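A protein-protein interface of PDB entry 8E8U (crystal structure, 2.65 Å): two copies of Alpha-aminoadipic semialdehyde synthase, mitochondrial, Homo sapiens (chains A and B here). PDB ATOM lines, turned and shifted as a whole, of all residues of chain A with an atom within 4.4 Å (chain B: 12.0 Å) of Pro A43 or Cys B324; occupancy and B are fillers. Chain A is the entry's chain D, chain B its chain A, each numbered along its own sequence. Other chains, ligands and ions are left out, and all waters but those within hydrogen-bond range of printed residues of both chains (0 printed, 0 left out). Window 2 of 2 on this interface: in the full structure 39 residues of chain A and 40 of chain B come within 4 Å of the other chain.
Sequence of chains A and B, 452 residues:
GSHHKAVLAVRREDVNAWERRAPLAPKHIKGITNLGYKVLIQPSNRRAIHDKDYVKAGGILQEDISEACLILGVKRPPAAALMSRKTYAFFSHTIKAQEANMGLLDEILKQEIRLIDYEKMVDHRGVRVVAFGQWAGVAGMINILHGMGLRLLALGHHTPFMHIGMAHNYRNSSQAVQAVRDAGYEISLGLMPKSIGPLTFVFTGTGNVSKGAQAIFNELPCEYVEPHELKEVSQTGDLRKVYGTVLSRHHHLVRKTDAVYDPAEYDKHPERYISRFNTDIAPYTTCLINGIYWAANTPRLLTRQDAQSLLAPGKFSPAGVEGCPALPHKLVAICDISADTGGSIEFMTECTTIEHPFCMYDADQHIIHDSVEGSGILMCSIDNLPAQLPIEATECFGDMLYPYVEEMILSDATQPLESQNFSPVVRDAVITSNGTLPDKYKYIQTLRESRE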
ATOM      1  N   ARG A  12      10.173 -11.813  34.170  1.00  0.00           N
ATOM      2  CA  ARG A  12       9.129 -10.955  33.634  1.00  0.00           C
ATOM      3  C   ARG A  12       9.297  -9.530  34.142  1.00  0.00           C
ATOM      4  O   ARG A  12       9.556  -9.304  35.327  1.00  0.00           O
ATOM      5  CB  ARG A  12       7.754 -11.493  34.025  1.00  0.00           C
ATOM      6  CG  ARG A  12       6.663 -10.439  34.122  1.00  0.00           C
ATOM      7  CD  ARG A  12       5.346 -11.048  34.578  1.00  0.00           C
ATOM      8  NE  ARG A  12       5.476 -12.467  34.903  1.00  0.00           N
ATOM      9  CZ  ARG A  12       5.653 -12.946  36.131  1.00  0.00           C
ATOM     10  NH1 ARG A  12       5.760 -14.255  36.320  1.00  0.00           N
ATOM     11  NH2 ARG A  12       5.726 -12.122  37.166  1.00  0.00           N
ATOM     12  N   ILE A  41      12.028 -19.316  30.657  1.00  0.00           N
ATOM     13  CA  ILE A  41      11.348 -18.087  30.269  1.00  0.00           C
ATOM     14  C   ILE A  41      10.131 -17.936  31.170  1.00  0.00           C
ATOM     15  O   ILE A  41       9.200 -18.749  31.109  1.00  0.00           O
ATOM     16  CB  ILE A  41      10.941 -18.091  28.791  1.00  0.00           C
ATOM     17  CG1 ILE A  41      12.166 -18.307  27.899  1.00  0.00           C
ATOM     18  CG2 ILE A  41      10.236 -16.789  28.433  1.00  0.00           C
ATOM     19  CD1 ILE A  41      13.176 -17.182  27.963  1.00  0.00           C
ATOM     20  N   GLN A  42      10.138 -16.908  32.006  1.00  0.00           N
ATOM     21  CA  GLN A  42       8.988 -16.644  32.858  1.00  0.00           C
ATOM     22  C   GLN A  42       7.858 -16.067  32.014  1.00  0.00           C
ATOM     23  O   GLN A  42       8.072 -15.088  31.288  1.00  0.00           O
ATOM     24  CB  GLN A  42       9.368 -15.681  33.980  1.00  0.00           C
ATOM     25  CG  GLN A  42       8.781 -16.045  35.335  1.00  0.00           C
ATOM     26  CD  GLN A  42       9.214 -15.094  36.434  1.00  0.00           C
ATOM     27  OE1 GLN A  42       9.740 -14.014  36.166  1.00  0.00           O
ATOM     28  NE2 GLN A  42       8.997 -15.496  37.681  1.00  0.00           N
ATOM     29  N   PRO A  43       6.657 -16.642  32.069  1.00  0.00           N
ATOM     30  CA  PRO A  43       5.568 -16.155  31.211  1.00  0.00           C
ATOM     31  C   PRO A  43       5.204 -14.715  31.540  1.00  0.00           C
ATOM     32  O   PRO A  43       5.178 -14.309  32.702  1.00  0.00           O
ATOM     33  CB  PRO A  43       4.414 -17.116  31.519  1.00  0.00           C
ATOM     34  CG  PRO A  43       4.742 -17.706  32.850  1.00  0.00           C
ATOM     35  CD  PRO A  43       6.237 -17.765  32.922  1.00  0.00           C
ATOM     36  N   SER A  44       4.923 -13.941  30.493  1.00  0.00           N
ATOM     37  CA  SER A  44       4.668 -12.512  30.646  1.00  0.00           C
ATOM     38  C   SER A  44       3.765 -12.058  29.510  1.00  0.00           C
ATOM     39  O   SER A  44       4.177 -12.072  28.346  1.00  0.00           O
ATOM     40  CB  SER A  44       5.977 -11.725  30.652  1.00  0.00           C
ATOM     41  OG  SER A  44       5.737 -10.333  30.773  1.00  0.00           O
ATOM     42  N   ASN A  45       2.537 -11.653  29.845  1.00  0.00           N
ATOM     43  CA  ASN A  45       1.667 -11.035  28.853  1.00  0.00           C
ATOM     44  C   ASN A  45       2.115  -9.622  28.501  1.00  0.00           C
ATOM     45  O   ASN A  45       1.667  -9.076  27.487  1.00  0.00           O
ATOM     46  CB  ASN A  45       0.221 -11.007  29.351  1.00  0.00           C
ATOM     47  CG  ASN A  45      -0.398 -12.389  29.434  1.00  0.00           C
ATOM     48  OD1 ASN A  45      -1.504 -12.554  29.947  1.00  0.00           O
ATOM     49  ND2 ASN A  45       0.317 -13.391  28.938  1.00  0.00           N
ATOM     50  N   ASP A  51       5.235 -15.378  24.198  1.00  0.00           N
ATOM     51  CA  ASP A  51       5.869 -16.513  24.861  1.00  0.00           C
ATOM     52  C   ASP A  51       6.121 -17.663  23.895  1.00  0.00           C
ATOM     53  O   ASP A  51       7.102 -18.400  24.049  1.00  0.00           O
ATOM     54  CB  ASP A  51       5.002 -16.985  26.028  1.00  0.00           C
ATOM     55  CG  ASP A  51       4.970 -15.991  27.172  1.00  0.00           C
ATOM     56  OD1 ASP A  51       5.895 -15.154  27.263  1.00  0.00           O
ATOM     57  OD2 ASP A  51       4.021 -16.047  27.982  1.00  0.00           O
ATOM     58  N   LEU A  61       8.828 -22.441  29.302  1.00  0.00           N
ATOM     59  CA  LEU A  61       7.897 -21.531  29.962  1.00  0.00           C
ATOM     60  C   LEU A  61       7.628 -22.044  31.371  1.00  0.00           C
ATOM     61  O   LEU A  61       7.043 -23.118  31.547  1.00  0.00           O
ATOM     62  CB  LEU A  61       6.603 -21.420  29.163  1.00  0.00           C
ATOM     63  CG  LEU A  61       6.523 -20.279  28.150  1.00  0.00           C
ATOM     64  CD1 LEU A  61       5.156 -20.266  27.490  1.00  0.00           C
ATOM     65  CD2 LEU A  61       6.811 -18.948  28.825  1.00  0.00           C
ATOM     66  N   GLN A  62       8.053 -21.283  32.378  1.00  0.00           N
ATOM     67  CA  GLN A  62       7.953 -21.738  33.758  1.00  0.00           C
ATOM     68  C   GLN A  62       7.878 -20.538  34.692  1.00  0.00           C
ATOM     69  O   GLN A  62       8.666 -19.597  34.561  1.00  0.00           O
ATOM     70  CB  GLN A  62       9.146 -22.635  34.111  1.00  0.00           C
ATOM     71  CG  GLN A  62       9.129 -23.215  35.511  1.00  0.00           C
ATOM     72  CD  GLN A  62      10.253 -24.211  35.730  1.00  0.00           C
ATOM     73  OE1 GLN A  62      10.910 -24.638  34.781  1.00  0.00           O
ATOM     74  NE2 GLN A  62      10.480 -24.584  36.984  1.00  0.00           N
ATOM     75  N   GLU A  63       6.928 -20.580  35.631  1.00  0.00           N
ATOM     76  CA  GLU A  63       6.815 -19.520  36.630  1.00  0.00           C
ATOM     77  C   GLU A  63       7.942 -19.574  37.651  1.00  0.00           C
ATOM     78  O   GLU A  63       8.514 -18.535  38.003  1.00  0.00           O
ATOM     79  CB  GLU A  63       5.462 -19.608  37.338  1.00  0.00           C
ATOM     80  CG  GLU A  63       5.148 -18.440  38.274  1.00  0.00           C
ATOM     81  CD  GLU A  63       5.129 -17.084  37.602  1.00  0.00           C
ATOM     82  OE1 GLU A  63       4.918 -17.015  36.374  1.00  0.00           O
ATOM     83  OE2 GLU A  63       5.329 -16.077  38.317  1.00  0.00           O
ATOM     84  N   LEU B 152      -5.879  -2.859  28.042  1.00  0.00           N
ATOM     85  CA  LEU B 152      -5.306  -4.178  28.290  1.00  0.00           C
ATOM     86  C   LEU B 152      -3.837  -4.088  28.690  1.00  0.00           C
ATOM     87  O   LEU B 152      -3.365  -4.879  29.514  1.00  0.00           O
ATOM     88  CB  LEU B 152      -5.472  -5.062  27.054  1.00  0.00           C
ATOM     89  CG  LEU B 152      -6.892  -5.570  26.796  1.00  0.00           C
ATOM     90  CD1 LEU B 152      -7.004  -6.194  25.416  1.00  0.00           C
ATOM     91  CD2 LEU B 152      -7.304  -6.564  27.873  1.00  0.00           C
ATOM     92  N   LEU B 153      -3.095  -3.141  28.108  1.00  0.00           N
ATOM     93  CA  LEU B 153      -1.703  -2.959  28.504  1.00  0.00           C
ATOM     94  C   LEU B 153      -1.600  -2.493  29.951  1.00  0.00           C
ATOM     95  O   LEU B 153      -0.701  -2.917  30.687  1.00  0.00           O
ATOM     96  CB  LEU B 153      -1.010  -1.973  27.565  1.00  0.00           C
ATOM     97  CG  LEU B 153       0.501  -1.827  27.752  1.00  0.00           C
ATOM     98  CD1 LEU B 153       1.192  -3.172  27.582  1.00  0.00           C
ATOM     99  CD2 LEU B 153       1.071  -0.803  26.786  1.00  0.00           C
ATOM    100  N   ALA B 154      -2.512  -1.612  30.377  1.00  0.00           N
ATOM    101  CA  ALA B 154      -2.536  -1.196  31.774  1.00  0.00           C
ATOM    102  C   ALA B 154      -2.860  -2.366  32.692  1.00  0.00           C
ATOM    103  O   ALA B 154      -2.390  -2.412  33.834  1.00  0.00           O
ATOM    104  CB  ALA B 154      -3.545  -0.065  31.973  1.00  0.00           C
ATOM    105  N   LEU B 155      -3.660  -3.317  32.209  1.00  0.00           N
ATOM    106  CA  LEU B 155      -3.954  -4.530  32.956  1.00  0.00           C
ATOM    107  C   LEU B 155      -2.831  -5.556  32.868  1.00  0.00           C
ATOM    108  O   LEU B 155      -2.911  -6.594  33.535  1.00  0.00           O
ATOM    109  CB  LEU B 155      -5.261  -5.150  32.453  1.00  0.00           C
ATOM    110  CG  LEU B 155      -6.547  -4.373  32.740  1.00  0.00           C
ATOM    111  CD1 LEU B 155      -7.743  -5.037  32.077  1.00  0.00           C
ATOM    112  CD2 LEU B 155      -6.771  -4.248  34.236  1.00  0.00           C
ATOM    113  N   GLY B 156      -1.798  -5.294  32.070  1.00  0.00           N
ATOM    114  CA  GLY B 156      -0.650  -6.169  31.977  1.00  0.00           C
ATOM    115  C   GLY B 156      -0.557  -7.013  30.723  1.00  0.00           C
ATOM    116  O   GLY B 156       0.267  -7.934  30.683  1.00  0.00           O
ATOM    117  N   HIS B 157      -1.364  -6.737  29.699  1.00  0.00           N
ATOM    118  CA  HIS B 157      -1.445  -7.583  28.514  1.00  0.00           C
ATOM    119  C   HIS B 157      -1.093  -6.774  27.274  1.00  0.00           C
ATOM    120  O   HIS B 157      -1.801  -5.822  26.929  1.00  0.00           O
ATOM    121  CB  HIS B 157      -2.843  -8.185  28.370  1.00  0.00           C
ATOM    122  CG  HIS B 157      -3.480  -8.556  29.672  1.00  0.00           C
ATOM    123  ND1 HIS B 157      -4.539  -7.855  30.208  1.00  0.00           N
ATOM    124  CD2 HIS B 157      -3.206  -9.550  30.550  1.00  0.00           C
ATOM    125  CE1 HIS B 157      -4.892  -8.402  31.356  1.00  0.00           C
ATOM    126  NE2 HIS B 157      -4.098  -9.432  31.588  1.00  0.00           N
ATOM    127  N   HIS B 158      -0.008  -7.155  26.604  1.00  0.00           N
ATOM    128  CA  HIS B 158       0.294  -6.621  25.283  1.00  0.00           C
ATOM    129  C   HIS B 158      -0.581  -7.316  24.249  1.00  0.00           C
ATOM    130  O   HIS B 158      -0.658  -8.549  24.219  1.00  0.00           O
ATOM    131  CB  HIS B 158       1.771  -6.815  24.945  1.00  0.00           C
ATOM    132  CG  HIS B 158       2.087  -6.619  23.494  1.00  0.00           C
ATOM    133  ND1 HIS B 158       2.336  -5.377  22.947  1.00  0.00           N
ATOM    134  CD2 HIS B 158       2.192  -7.505  22.476  1.00  0.00           C
ATOM    135  CE1 HIS B 158       2.582  -5.509  21.656  1.00  0.00           C
ATOM    136  NE2 HIS B 158       2.501  -6.790  21.344  1.00  0.00           N
ATOM    137  N   THR B 159      -1.235  -6.534  23.401  1.00  0.00           N
ATOM    138  CA  THR B 159      -2.169  -7.057  22.418  1.00  0.00           C
ATOM    139  C   THR B 159      -1.931  -6.374  21.080  1.00  0.00           C
ATOM    140  O   THR B 159      -1.366  -5.277  21.028  1.00  0.00           O
ATOM    141  CB  THR B 159      -3.626  -6.842  22.851  1.00  0.00           C
ATOM    142  OG1 THR B 159      -3.887  -5.438  22.981  1.00  0.00           O
ATOM    143  CG2 THR B 159      -3.905  -7.538  24.176  1.00  0.00           C
ATOM    144  N   GLY B 190      -2.103 -15.968  16.527  1.00  0.00           N
ATOM    145  CA  GLY B 190      -2.063 -16.403  17.906  1.00  0.00           C
ATOM    146  C   GLY B 190      -1.259 -15.521  18.829  1.00  0.00           C
ATOM    147  O   GLY B 190      -0.865 -15.979  19.908  1.00  0.00           O
ATOM    148  N   LEU B 191      -1.006 -14.269  18.450  1.00  0.00           N
ATOM    149  CA  LEU B 191      -0.216 -13.370  19.281  1.00  0.00           C
ATOM    150  C   LEU B 191      -1.027 -12.737  20.402  1.00  0.00           C
ATOM    151  O   LEU B 191      -0.463 -11.983  21.203  1.00  0.00           O
ATOM    152  CB  LEU B 191       0.420 -12.278  18.417  1.00  0.00           C
ATOM    153  CG  LEU B 191       1.346 -12.771  17.303  1.00  0.00           C
ATOM    154  CD1 LEU B 191       1.955 -11.596  16.548  1.00  0.00           C
ATOM    155  CD2 LEU B 191       2.429 -13.678  17.868  1.00  0.00           C
ATOM    156  N   MET B 192      -2.323 -13.025  20.480  1.00  0.00           N
ATOM    157  CA  MET B 192      -3.128 -12.546  21.588  1.00  0.00           C
ATOM    158  C   MET B 192      -2.767 -13.314  22.858  1.00  0.00           C
ATOM    159  O   MET B 192      -2.446 -14.504  22.804  1.00  0.00           O
ATOM    160  CB  MET B 192      -4.613 -12.710  21.280  1.00  0.00           C
ATOM    161  CG  MET B 192      -5.182 -11.643  20.362  1.00  0.00           C
ATOM    162  SD  MET B 192      -5.594 -10.127  21.243  1.00  0.00           S
ATOM    163  CE  MET B 192      -7.021 -10.669  22.175  1.00  0.00           C
ATOM    164  N   PRO B 193      -2.813 -12.657  24.016  1.00  0.00           N
ATOM    165  CA  PRO B 193      -2.528 -13.359  25.275  1.00  0.00           C
ATOM    166  C   PRO B 193      -3.624 -14.360  25.615  1.00  0.00           C
ATOM    167  O   PRO B 193      -4.816 -14.059  25.516  1.00  0.00           O
ATOM    168  CB  PRO B 193      -2.454 -12.228  26.307  1.00  0.00           C
ATOM    169  CG  PRO B 193      -3.253 -11.119  25.710  1.00  0.00           C
ATOM    170  CD  PRO B 193      -3.065 -11.221  24.223  1.00  0.00           C
ATOM    171  N   LYS B 194      -3.206 -15.566  26.008  1.00  0.00           N
ATOM    172  CA  LYS B 194      -4.158 -16.641  26.268  1.00  0.00           C
ATOM    173  C   LYS B 194      -4.988 -16.378  27.518  1.00  0.00           C
ATOM    174  O   LYS B 194      -6.141 -16.816  27.595  1.00  0.00           O
ATOM    175  CB  LYS B 194      -3.420 -17.973  26.418  1.00  0.00           C
ATOM    176  CG  LYS B 194      -2.512 -18.359  25.259  1.00  0.00           C
ATOM    177  CD  LYS B 194      -3.238 -18.290  23.933  1.00  0.00           C
ATOM    178  CE  LYS B 194      -2.311 -18.561  22.767  1.00  0.00           C
ATOM    179  NZ  LYS B 194      -3.027 -18.432  21.469  1.00  0.00           N
ATOM    180  N   SER B 195      -4.425 -15.670  28.501  1.00  0.00           N
ATOM    181  CA  SER B 195      -5.068 -15.572  29.807  1.00  0.00           C
ATOM    182  C   SER B 195      -6.333 -14.719  29.775  1.00  0.00           C
ATOM    183  O   SER B 195      -7.234 -14.927  30.596  1.00  0.00           O
ATOM    184  CB  SER B 195      -4.082 -15.011  30.830  1.00  0.00           C
ATOM    185  OG  SER B 195      -3.779 -13.656  30.555  1.00  0.00           O
ATOM    186  N   ILE B 196      -6.426 -13.761  28.851  1.00  0.00           N
ATOM    187  CA  ILE B 196      -7.612 -12.911  28.812  1.00  0.00           C
ATOM    188  C   ILE B 196      -8.808 -13.614  28.187  1.00  0.00           C
ATOM    189  O   ILE B 196      -9.952 -13.211  28.433  1.00  0.00           O
ATOM    190  CB  ILE B 196      -7.335 -11.595  28.065  1.00  0.00           C
ATOM    191  CG1 ILE B 196      -7.112 -11.853  26.575  1.00  0.00           C
ATOM    192  CG2 ILE B 196      -6.138 -10.879  28.674  1.00  0.00           C
ATOM    193  CD1 ILE B 196      -6.853 -10.597  25.780  1.00  0.00           C
ATOM    194  N   GLY B 197      -8.583 -14.650  27.382  1.00  0.00           N
ATOM    195  CA  GLY B 197      -9.663 -15.408  26.801  1.00  0.00           C
ATOM    196  C   GLY B 197     -10.193 -14.752  25.543  1.00  0.00           C
ATOM    197  O   GLY B 197      -9.694 -13.712  25.101  1.00  0.00           O
ATOM    198  N   LEU B 239      -8.997 -18.437  20.501  1.00  0.00           N
ATOM    199  CA  LEU B 239      -8.215 -17.257  20.840  1.00  0.00           C
ATOM    200  C   LEU B 239      -7.599 -16.586  19.620  1.00  0.00           C
ATOM    201  O   LEU B 239      -7.078 -15.472  19.740  1.00  0.00           O
ATOM    202  CB  LEU B 239      -7.124 -17.643  21.839  1.00  0.00           C
ATOM    203  CG  LEU B 239      -7.710 -18.308  23.086  1.00  0.00           C
ATOM    204  CD1 LEU B 239      -6.639 -18.755  24.056  1.00  0.00           C
ATOM    205  CD2 LEU B 239      -8.675 -17.357  23.767  1.00  0.00           C
ATOM    206  N   GLU B 322       0.532 -16.330  37.627  1.00  0.00           N
ATOM    207  CA  GLU B 322       0.826 -15.032  38.220  1.00  0.00           C
ATOM    208  C   GLU B 322       1.227 -14.028  37.145  1.00  0.00           C
ATOM    209  O   GLU B 322       0.804 -12.873  37.161  1.00  0.00           O
ATOM    210  CB  GLU B 322       1.939 -15.155  39.262  1.00  0.00           C
ATOM    211  CG  GLU B 322       1.686 -16.210  40.326  1.00  0.00           C
ATOM    212  CD  GLU B 322       2.734 -16.191  41.421  1.00  0.00           C
ATOM    213  OE1 GLU B 322       3.808 -15.588  41.208  1.00  0.00           O
ATOM    214  OE2 GLU B 322       2.487 -16.783  42.493  1.00  0.00           O
ATOM    215  N   GLY B 323       2.051 -14.495  36.204  1.00  0.00           N
ATOM    216  CA  GLY B 323       2.499 -13.642  35.119  1.00  0.00           C
ATOM    217  C   GLY B 323       1.432 -13.368  34.081  1.00  0.00           C
ATOM    218  O   GLY B 323       1.479 -12.345  33.392  1.00  0.00           O
ATOM    219  N   CYS B 324       0.461 -14.273  33.950  1.00  0.00           N
ATOM    220  CA  CYS B 324      -0.599 -14.182  32.950  1.00  0.00           C
ATOM    221  C   CYS B 324      -1.921 -14.048  33.693  1.00  0.00           C
ATOM    222  O   CYS B 324      -2.625 -15.044  33.916  1.00  0.00           O
ATOM    223  CB  CYS B 324      -0.603 -15.403  32.033  1.00  0.00           C
ATOM    224  SG  CYS B 324       1.034 -15.914  31.464  1.00  0.00           S
ATOM    225  N   PRO B 325      -2.288 -12.836  34.096  1.00  0.00           N
ATOM    226  CA  PRO B 325      -3.533 -12.661  34.845  1.00  0.00           C
ATOM    227  C   PRO B 325      -4.744 -12.685  33.932  1.00  0.00           C
ATOM    228  O   PRO B 325      -4.678 -12.340  32.749  1.00  0.00           O
ATOM    229  CB  PRO B 325      -3.365 -11.280  35.488  1.00  0.00           C
ATOM    230  CG  PRO B 325      -2.459 -10.541  34.554  1.00  0.00           C
ATOM    231  CD  PRO B 325      -1.602 -11.557  33.842  1.00  0.00           C
ATOM    232  N   ALA B 326      -5.867 -13.104  34.505  1.00  0.00           N
ATOM    233  CA  ALA B 326      -7.130 -13.039  33.797  1.00  0.00           C
ATOM    234  C   ALA B 326      -7.731 -11.647  33.946  1.00  0.00           C
ATOM    235  O   ALA B 326      -7.322 -10.854  34.799  1.00  0.00           O
ATOM    236  CB  ALA B 326      -8.099 -14.099  34.320  1.00  0.00           C
ATOM    237  N   LEU B 327      -8.701 -11.347  33.093  1.00  0.00           N
ATOM    238  CA  LEU B 327      -9.391 -10.073  33.200  1.00  0.00           C
ATOM    239  C   LEU B 327     -10.103  -9.990  34.548  1.00  0.00           C
ATOM    240  O   LEU B 327     -10.597 -11.007  35.051  1.00  0.00           O
ATOM    241  CB  LEU B 327     -10.395  -9.905  32.059  1.00  0.00           C
ATOM    242  CG  LEU B 327      -9.789  -9.759  30.663  1.00  0.00           C
ATOM    243  CD1 LEU B 327     -10.881  -9.665  29.611  1.00  0.00           C
ATOM    244  CD2 LEU B 327      -8.873  -8.547  30.605  1.00  0.00           C
ATOM    245  N   PRO B 328     -10.167  -8.808  35.167  1.00  0.00           N
ATOM    246  CA  PRO B 328     -10.929  -8.699  36.422  1.00  0.00           C
ATOM    247  C   PRO B 328     -12.410  -8.957  36.225  1.00  0.00           C
ATOM    248  O   PRO B 328     -13.046  -9.604  37.067  1.00  0.00           O
ATOM    249  CB  PRO B 328     -10.645  -7.261  36.880  1.00  0.00           C
ATOM    250  CG  PRO B 328     -10.268  -6.529  35.633  1.00  0.00           C
ATOM    251  CD  PRO B 328      -9.563  -7.527  34.762  1.00  0.00           C
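No position is printed for both chains. Of the 12 pairs that touch across the chains among the printed residues, none has its exchanged pair printed and touching as well.
O of Pro B325 lies within hydrogen-bond range of NE2 of His B157 (3.2 Å). The side-chain amide oxygen (OE1) of Gln A42 lies within hydrogen-bond range of the backbone NH (N) of Arg A12 (3.0 Å). The side-chain carboxylate of Glu A63 lies within salt-bridge range of the guanidinium group of Arg A12 (2.7 Å). NE2 of Gln A42 is in hydrogen-bond range of O of Glu A63 (3.1 Å). The backbone carbonyl oxygen (O) of Pro A43 lies within hydrogen-bond range of the guanidinium group (NE) of Arg A12, 2.9 Å away. O of Leu B152 sits at hydrogen-bond distance from N of His B157, at 2.7 Å.
Of the 24 printed residues of chain B, 8 touch a printed residue of chain A. Hydrophobic or aromatic side chains of chain B that line the printed part of chain A: His B157, His B158 and Pro B193. Among the printed residues, no Asp or Glu carboxylate lies within 4 Å of a Lys or Arg side-chain nitrogen of the other chain.
CA of Gly B323 touches NE of Arg A12, 3.2 Å away. CA of Gly B323 touches O of Pro A43 (3.7 Å). CB of Pro A43 touches SG of Cys B324, at 3.6 Å. Gly B156 touches Asn A45. His B157 touches Asn A45. Asn A45 touches Pro B193. N of Asn A45 touches O of Gly B323, 3.8 Å away. Gly B323 touches Glu A63 (N to OE1, 3.8 Å).
Of chain B, only Gly B323 (3.7 Å) and Cys B324 (3.6 Å) come within 4 Å of Pro A43. Cys B324 touches just these residues of chain A: Pro A43 (3.6 Å) and Asn A45 (3.5 Å). No residue of chain B comes within 4 Å of Ile A41. No residue of chain B comes within 4 Å of Gln A42. No residue of chain B comes within 4 Å of Ser A44. No residue of chain B comes within 4 Å of Asp A51. No residue of chain B comes within 4 Å of Leu A61. Of the printed residues of chain A, Gly B156 touches Asn A45. Of the printed residues of chain A, Gly B323 touches Arg A12 (3.2 Å), Pro A43 (3.7 Å), Asn A45 (3.8 Å) and Glu A63 (3.8 Å). Leu B191 touches none of the printed residues of chain A. The nearest residue of chain B that does not touch Pro A43 is Glu B322 (6.0 Å). The nearest printed residue of chain A that does not touch Cys B324 is Ser A44 (4.5 Å). The nearest printed residue of chain A that does not touch Glu B322 is Arg A12 (4.6 Å).
The side-chain carboxylate of Glu A63 sits close to the side-chain carboxylate of Glu B322 (3.3 Å). The side-chain amide oxygen (OD1) of Asn A45 is in hydrogen-bond range of the side-chain hydroxyl (OG) of Ser B195, at 2.6 Å. O of Asn A45 lies within hydrogen-bond range of N of His B158, at 2.7 Å. The side-chain sulfur of Cys B324 lies within hydrogen-bond range of the side-chain amide nitrogen of Asn A45 (3.6 Å).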
